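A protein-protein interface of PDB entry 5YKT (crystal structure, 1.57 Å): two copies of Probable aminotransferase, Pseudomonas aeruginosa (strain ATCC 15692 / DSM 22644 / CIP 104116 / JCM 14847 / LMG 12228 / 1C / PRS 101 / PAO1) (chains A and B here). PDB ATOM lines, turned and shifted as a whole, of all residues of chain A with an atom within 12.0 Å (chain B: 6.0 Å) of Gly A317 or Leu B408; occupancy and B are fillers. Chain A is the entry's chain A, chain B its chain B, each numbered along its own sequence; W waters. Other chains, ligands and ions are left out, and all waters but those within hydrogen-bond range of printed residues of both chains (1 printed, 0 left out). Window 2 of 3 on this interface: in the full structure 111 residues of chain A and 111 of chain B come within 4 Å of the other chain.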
ATOM      1  N   PRO A 312      20.729  37.869   5.149  1.00  0.00           N
ATOM      2  CA  PRO A 312      21.895  37.109   5.554  1.00  0.00           C
ATOM      3  C   PRO A 312      22.418  36.158   4.493  1.00  0.00           C
ATOM      4  O   PRO A 312      21.681  35.724   3.597  1.00  0.00           O
ATOM      5  CB  PRO A 312      21.416  36.304   6.762  1.00  0.00           C
ATOM      6  CG  PRO A 312      20.225  37.035   7.242  1.00  0.00           C
ATOM      7  CD  PRO A 312      19.588  37.642   6.055  1.00  0.00           C
ATOM      8  N   HIS A 313      23.694  35.845   4.613  1.00  0.00           N
ATOM      9  CA  HIS A 313      24.300  34.803   3.802  1.00  0.00           C
ATOM     10  C   HIS A 313      23.490  33.525   3.968  1.00  0.00           C
ATOM     11  O   HIS A 313      23.016  33.218   5.057  1.00  0.00           O
ATOM     12  CB  HIS A 313      25.749  34.609   4.182  1.00  0.00           C
ATOM     13  CG  HIS A 313      26.584  35.801   3.861  1.00  0.00           C
ATOM     14  ND1 HIS A 313      26.966  36.100   2.574  1.00  0.00           N
ATOM     15  CD2 HIS A 313      27.051  36.797   4.642  1.00  0.00           C
ATOM     16  CE1 HIS A 313      27.677  37.210   2.586  1.00  0.00           C
ATOM     17  NE2 HIS A 313      27.745  37.653   3.826  1.00  0.00           N
ATOM     18  N   PHE A 314      23.305  32.816   2.866  1.00  0.00           N
ATOM     19  CA  PHE A 314      22.403  31.657   2.830  1.00  0.00           C
ATOM     20  C   PHE A 314      22.929  30.528   3.678  1.00  0.00           C
ATOM     21  O   PHE A 314      24.112  30.250   3.685  1.00  0.00           O
ATOM     22  CB  PHE A 314      22.228  31.197   1.380  1.00  0.00           C
ATOM     23  CG  PHE A 314      20.983  30.393   1.138  1.00  0.00           C
ATOM     24  CD1 PHE A 314      19.753  31.030   0.997  1.00  0.00           C
ATOM     25  CD2 PHE A 314      21.063  29.035   0.959  1.00  0.00           C
ATOM     26  CE1 PHE A 314      18.602  30.309   0.729  1.00  0.00           C
ATOM     27  CE2 PHE A 314      19.916  28.299   0.697  1.00  0.00           C
ATOM     28  CZ  PHE A 314      18.694  28.931   0.571  1.00  0.00           C
ATOM     29  N   ARG A 315      22.023  29.884   4.424  1.00  0.00           N
ATOM     30  CA  ARG A 315      22.384  28.815   5.354  1.00  0.00           C
ATOM     31  C   ARG A 315      22.009  27.440   4.776  1.00  0.00           C
ATOM     32  O   ARG A 315      21.065  27.338   3.976  1.00  0.00           O
ATOM     33  CB  ARG A 315      21.686  29.035   6.690  1.00  0.00           C
ATOM     34  CG  ARG A 315      22.143  30.298   7.422  1.00  0.00           C
ATOM     35  CD  ARG A 315      21.329  30.563   8.690  1.00  0.00           C
ATOM     36  NE  ARG A 315      21.977  31.504   9.628  1.00  0.00           N
ATOM     37  CZ  ARG A 315      21.781  32.832   9.694  1.00  0.00           C
ATOM     38  NH1 ARG A 315      20.920  33.464   8.890  1.00  0.00           N
ATOM     39  NH2 ARG A 315      22.437  33.542  10.626  1.00  0.00           N
ATOM     40  N   PRO A 316      22.746  26.382   5.170  1.00  0.00           N
ATOM     41  CA  PRO A 316      22.479  25.046   4.628  1.00  0.00           C
ATOM     42  C   PRO A 316      21.049  24.619   4.900  1.00  0.00           C
ATOM     43  O   PRO A 316      20.598  24.698   6.043  1.00  0.00           O
ATOM     44  CB  PRO A 316      23.448  24.139   5.407  1.00  0.00           C
ATOM     45  CG  PRO A 316      24.500  25.040   5.932  1.00  0.00           C
ATOM     46  CD  PRO A 316      23.855  26.364   6.141  1.00  0.00           C
ATOM     47  N   GLY A 317      20.326  24.199   3.859  1.00  0.00           N
ATOM     48  CA  GLY A 317      18.951  23.746   4.016  1.00  0.00           C
ATOM     49  C   GLY A 317      17.888  24.821   4.139  1.00  0.00           C
ATOM     50  O   GLY A 317      16.715  24.514   4.307  1.00  0.00           O
ATOM     51  N   GLN A 318      18.290  26.089   4.039  1.00  0.00           N
ATOM     52  CA  GLN A 318      17.353  27.205   4.088  1.00  0.00           C
ATOM     53  C   GLN A 318      16.409  27.150   2.879  1.00  0.00           C
ATOM     54  O   GLN A 318      16.796  26.688   1.785  1.00  0.00           O
ATOM     55  CB  GLN A 318      18.157  28.519   4.099  1.00  0.00           C
ATOM     56  CG  GLN A 318      17.325  29.775   4.128  1.00  0.00           C
ATOM     57  CD  GLN A 318      18.168  31.040   4.189  1.00  0.00           C
ATOM     58  OE1 GLN A 318      19.327  31.018   4.626  1.00  0.00           O
ATOM     59  NE2 GLN A 318      17.577  32.153   3.773  1.00  0.00           N
ATOM     60  N   ALA A 319      15.174  27.617   3.062  1.00  0.00           N
ATOM     61  CA  ALA A 319      14.245  27.727   1.947  1.00  0.00           C
ATOM     62  C   ALA A 319      14.833  28.635   0.862  1.00  0.00           C
ATOM     63  O   ALA A 319      15.233  29.776   1.132  1.00  0.00           O
ATOM     64  CB  ALA A 319      12.894  28.258   2.405  1.00  0.00           C
ATOM     65  N   ILE A 320      14.878  28.111  -0.359  1.00  0.00           N
ATOM     66  CA  ILE A 320      15.282  28.884  -1.540  1.00  0.00           C
ATOM     67  C   ILE A 320      14.442  30.163  -1.700  1.00  0.00           C
ATOM     68  O   ILE A 320      13.243  30.160  -1.448  1.00  0.00           O
ATOM     69  CB  ILE A 320      15.206  27.964  -2.809  1.00  0.00           C
ATOM     70  CG1 ILE A 320      16.605  27.438  -3.148  1.00  0.00           C
ATOM     71  CG2 ILE A 320      14.587  28.644  -4.035  1.00  0.00           C
ATOM     72  CD1 ILE A 320      17.262  26.592  -2.090  1.00  0.00           C
ATOM     73  N   ASN A 321      15.086  31.248  -2.131  1.00  0.00           N
ATOM     74  CA  ASN A 321      14.367  32.490  -2.400  1.00  0.00           C
ATOM     75  C   ASN A 321      15.220  33.411  -3.263  1.00  0.00           C
ATOM     76  O   ASN A 321      16.414  33.520  -3.058  1.00  0.00           O
ATOM     77  CB  ASN A 321      13.978  33.191  -1.083  1.00  0.00           C
ATOM     78  CG  ASN A 321      12.769  34.116  -1.231  1.00  0.00           C
ATOM     79  OD1 ASN A 321      12.452  34.589  -2.319  1.00  0.00           O
ATOM     80  ND2 ASN A 321      12.069  34.353  -0.127  1.00  0.00           N
ATOM     81  N   PHE A 323      14.377  36.633  -3.285  1.00  0.00           N
ATOM     82  CA  PHE A 323      14.305  37.857  -2.485  1.00  0.00           C
ATOM     83  C   PHE A 323      13.927  39.096  -3.305  1.00  0.00           C
ATOM     84  O   PHE A 323      14.171  40.224  -2.873  1.00  0.00           O
ATOM     85  CB  PHE A 323      15.601  38.087  -1.683  1.00  0.00           C
ATOM     86  CG  PHE A 323      15.991  36.914  -0.836  1.00  0.00           C
ATOM     87  CD1 PHE A 323      15.269  36.605   0.316  1.00  0.00           C
ATOM     88  CD2 PHE A 323      17.092  36.130  -1.161  1.00  0.00           C
ATOM     89  CE1 PHE A 323      15.640  35.536   1.115  1.00  0.00           C
ATOM     90  CE2 PHE A 323      17.451  35.053  -0.362  1.00  0.00           C
ATOM     91  CZ  PHE A 323      16.726  34.765   0.772  1.00  0.00           C
ATOM     92  N   LEU B   9      12.888  13.355   9.485  1.00  0.00           N
ATOM     93  CA  LEU B   9      13.753  14.525   9.276  1.00  0.00           C
ATOM     94  C   LEU B   9      15.066  14.443  10.055  1.00  0.00           C
ATOM     95  O   LEU B   9      16.040  15.083   9.669  1.00  0.00           O
ATOM     96  CB  LEU B   9      13.022  15.841   9.581  1.00  0.00           C
ATOM     97  CG  LEU B   9      11.935  16.279   8.582  1.00  0.00           C
ATOM     98  CD1 LEU B   9      11.298  17.581   9.051  1.00  0.00           C
ATOM     99  CD2 LEU B   9      12.459  16.437   7.158  1.00  0.00           C
ATOM    100  N   VAL B  12      17.251  12.497   7.787  1.00  0.00           N
ATOM    101  CA  VAL B  12      17.604  13.416   6.702  1.00  0.00           C
ATOM    102  C   VAL B  12      18.761  14.294   7.153  1.00  0.00           C
ATOM    103  O   VAL B  12      19.725  14.453   6.420  1.00  0.00           O
ATOM    104  CB  VAL B  12      16.418  14.284   6.201  1.00  0.00           C
ATOM    105  CG1 VAL B  12      16.873  15.246   5.089  1.00  0.00           C
ATOM    106  CG2 VAL B  12      15.314  13.401   5.650  1.00  0.00           C
ATOM    107  N   GLU B  13      18.669  14.844   8.361  1.00  0.00           N
ATOM    108  CA  GLU B  13      19.748  15.663   8.926  1.00  0.00           C
ATOM    109  C   GLU B  13      21.066  14.899   9.054  1.00  0.00           C
ATOM    110  O   GLU B  13      22.117  15.433   8.726  1.00  0.00           O
ATOM    111  CB  GLU B  13      19.334  16.232  10.301  1.00  0.00           C
ATOM    112  CG  GLU B  13      20.423  16.955  11.084  1.00  0.00           C
ATOM    113  CD  GLU B  13      20.858  18.289  10.484  1.00  0.00           C
ATOM    114  OE1 GLU B  13      20.329  18.713   9.424  1.00  0.00           O
ATOM    115  OE2 GLU B  13      21.739  18.937  11.096  1.00  0.00           O
ATOM    116  N   PHE B  16      22.473  14.451   5.607  1.00  0.00           N
ATOM    117  CA  PHE B  16      22.877  15.765   5.122  1.00  0.00           C
ATOM    118  C   PHE B  16      24.224  16.196   5.695  1.00  0.00           C
ATOM    119  O   PHE B  16      25.091  16.662   4.977  1.00  0.00           O
ATOM    120  CB  PHE B  16      21.791  16.797   5.434  1.00  0.00           C
ATOM    121  CG  PHE B  16      22.009  18.151   4.818  1.00  0.00           C
ATOM    122  CD1 PHE B  16      22.405  18.302   3.482  1.00  0.00           C
ATOM    123  CD2 PHE B  16      21.745  19.298   5.558  1.00  0.00           C
ATOM    124  CE1 PHE B  16      22.571  19.556   2.923  1.00  0.00           C
ATOM    125  CE2 PHE B  16      21.913  20.553   4.998  1.00  0.00           C
ATOM    126  CZ  PHE B  16      22.306  20.682   3.681  1.00  0.00           C
ATOM    127  N   ASN B 406      10.217  21.400   1.056  1.00  0.00           N
ATOM    128  CA  ASN B 406      11.003  21.347   2.290  1.00  0.00           C
ATOM    129  C   ASN B 406      12.473  21.528   1.959  1.00  0.00           C
ATOM    130  O   ASN B 406      13.051  20.719   1.234  1.00  0.00           O
ATOM    131  CB  ASN B 406      10.786  20.021   2.999  1.00  0.00           C
ATOM    132  CG  ASN B 406      11.510  19.949   4.328  1.00  0.00           C
ATOM    133  OD1 ASN B 406      12.693  19.622   4.392  1.00  0.00           O
ATOM    134  ND2 ASN B 406      10.802  20.252   5.397  1.00  0.00           N
ATOM    135  N   GLY B 407      13.072  22.583   2.497  1.00  0.00           N
ATOM    136  CA  GLY B 407      14.443  22.957   2.170  1.00  0.00           C
ATOM    137  C   GLY B 407      15.471  21.907   2.548  1.00  0.00           C
ATOM    138  O   GLY B 407      16.426  21.698   1.807  1.00  0.00           O
ATOM    139  N   LEU B 408      15.272  21.248   3.692  1.00  0.00           N
ATOM    140  CA  LEU B 408      16.237  20.267   4.189  1.00  0.00           C
ATOM    141  C   LEU B 408      16.244  19.013   3.318  1.00  0.00           C
ATOM    142  O   LEU B 408      17.307  18.535   2.937  1.00  0.00           O
ATOM    143  CB  LEU B 408      15.943  19.881   5.640  1.00  0.00           C
ATOM    144  CG  LEU B 408      16.823  18.771   6.233  1.00  0.00           C
ATOM    145  CD1 LEU B 408      18.300  19.110   6.113  1.00  0.00           C
ATOM    146  CD2 LEU B 408      16.423  18.447   7.662  1.00  0.00           C
ATOM    147  N   ILE B 409      15.060  18.474   3.038  1.00  0.00           N
ATOM    148  CA  ILE B 409      14.960  17.280   2.200  1.00  0.00           C
ATOM    149  C   ILE B 409      15.518  17.585   0.812  1.00  0.00           C
ATOM    150  O   ILE B 409      16.283  16.792   0.260  1.00  0.00           O
ATOM    151  CB  ILE B 409      13.513  16.752   2.088  1.00  0.00           C
ATOM    152  CG1 ILE B 409      13.030  16.246   3.445  1.00  0.00           C
ATOM    153  CG2 ILE B 409      13.430  15.620   1.059  1.00  0.00           C
ATOM    154  CD1 ILE B 409      11.529  15.997   3.516  1.00  0.00           C
ATOM    155  N   GLU B 410      15.143  18.737   0.263  1.00  0.00           N
ATOM    156  CA  GLU B 410      15.615  19.136  -1.060  1.00  0.00           C
ATOM    157  C   GLU B 410      17.132  19.271  -1.094  1.00  0.00           C
ATOM    158  O   GLU B 410      17.778  18.763  -2.013  1.00  0.00           O
ATOM    159  CB  GLU B 410      14.967  20.458  -1.488  1.00  0.00           C
ATOM    160  CG  GLU B 410      13.486  20.296  -1.790  1.00  0.00           C
ATOM    161  CD  GLU B 410      12.706  21.587  -1.785  1.00  0.00           C
ATOM    162  OE1 GLU B 410      13.276  22.682  -2.047  1.00  0.00           O
ATOM    163  OE2 GLU B 410      11.481  21.489  -1.545  1.00  0.00           O
ATOM    164  N   ALA B 411      17.701  19.974  -0.114  1.00  0.00           N
ATOM    165  CA  ALA B 411      19.158  20.159  -0.047  1.00  0.00           C
ATOM    166  C   ALA B 411      19.891  18.825   0.076  1.00  0.00           C
ATOM    167  O   ALA B 411      20.910  18.609  -0.584  1.00  0.00           O
ATOM    168  CB  ALA B 411      19.523  21.053   1.131  1.00  0.00           C
ATOM    169  N   CYS B 412      19.368  17.930   0.905  1.00  0.00           N
ATOM    170  CA  CYS B 412      19.980  16.610   1.091  1.00  0.00           C
ATOM    171  C   CYS B 412      19.984  15.791  -0.205  1.00  0.00           C
ATOM    172  O   CYS B 412      21.023  15.233  -0.581  1.00  0.00           O
ATOM    173  CB  CYS B 412      19.255  15.824   2.172  1.00  0.00           C
ATOM    174  SG  CYS B 412      20.116  14.308   2.625  1.00  0.00           S
ATOM    175  N   LEU B 413      18.837  15.721  -0.878  1.00  0.00           N
ATOM    176  CA  LEU B 413      18.749  14.983  -2.143  1.00  0.00           C
ATOM    177  C   LEU B 413      19.685  15.594  -3.185  1.00  0.00           C
ATOM    178  O   LEU B 413      20.424  14.850  -3.864  1.00  0.00           O
ATOM    179  CB  LEU B 413      17.319  14.973  -2.699  1.00  0.00           C
ATOM    180  CG  LEU B 413      16.243  14.172  -1.976  1.00  0.00           C
ATOM    181  CD1 LEU B 413      14.918  14.410  -2.700  1.00  0.00           C
ATOM    182  CD2 LEU B 413      16.603  12.696  -1.945  1.00  0.00           C
HETATM  183  O   HOH W   1      14.685  25.094  -0.918  1.00  0.00           O
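OD1 of Asn B406 is in hydrogen-bond range of N of Leu B408 (3.1 Å).
Phe B16 touches Pro A316. Gly A317 touches Gly B407 (O to C, 3.4 Å). Gly A317 touches Leu B408. Gly A317 touches Ala B411.
Printed residues of chain B within 4 Å of Gly A317: Gly B407 (3.4 Å), Leu B408 (3.6 Å) and Ala B411 (3.99 Å). Leu B408 touches just one residue of chain A: Gly A317. No residue of chain A comes within 4 Å of Val B12. No residue of chain A comes within 4 Å of Glu B13. Phe B16 touches just one residue of chain A: Pro A316 (3.9 Å). No residue of chain A comes within 4 Å of Asn B406. No residue of chain A comes within 4 Å of Ile B409. No residue of chain A comes within 4 Å of Glu B410. No residue of chain A comes within 4 Å of Cys B412. Of the printed residues of chain A, Ala B411 touches Gly A317 (3.99 Å). Of the printed residues of chain B, Pro A316 touches Phe B16. Ile A320 touches none of the printed residues of chain B. The nearest printed residue of chain B that does not touch Gly A317 is Phe B16 (4.04 Å).
Hydrophobic or aromatic side chains of chain A within 4 Å of the printed part of chain B: Pro A316. Hydrophobic or aromatic side chains of chain B within 4 Å of the printed part of chain A: Phe B16 and Ala B411. Among the printed residues, 4 pairs touch across the chains.
No position is printed for both chains. Of the 4 pairs that touch across the chains among the printed residues, none has its exchanged pair printed and touching as well.
Water W1 bridges the side-chain carboxylate of Glu B410 (3.0 Å) and the backbone NH of Ile A320 (3.1 Å).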
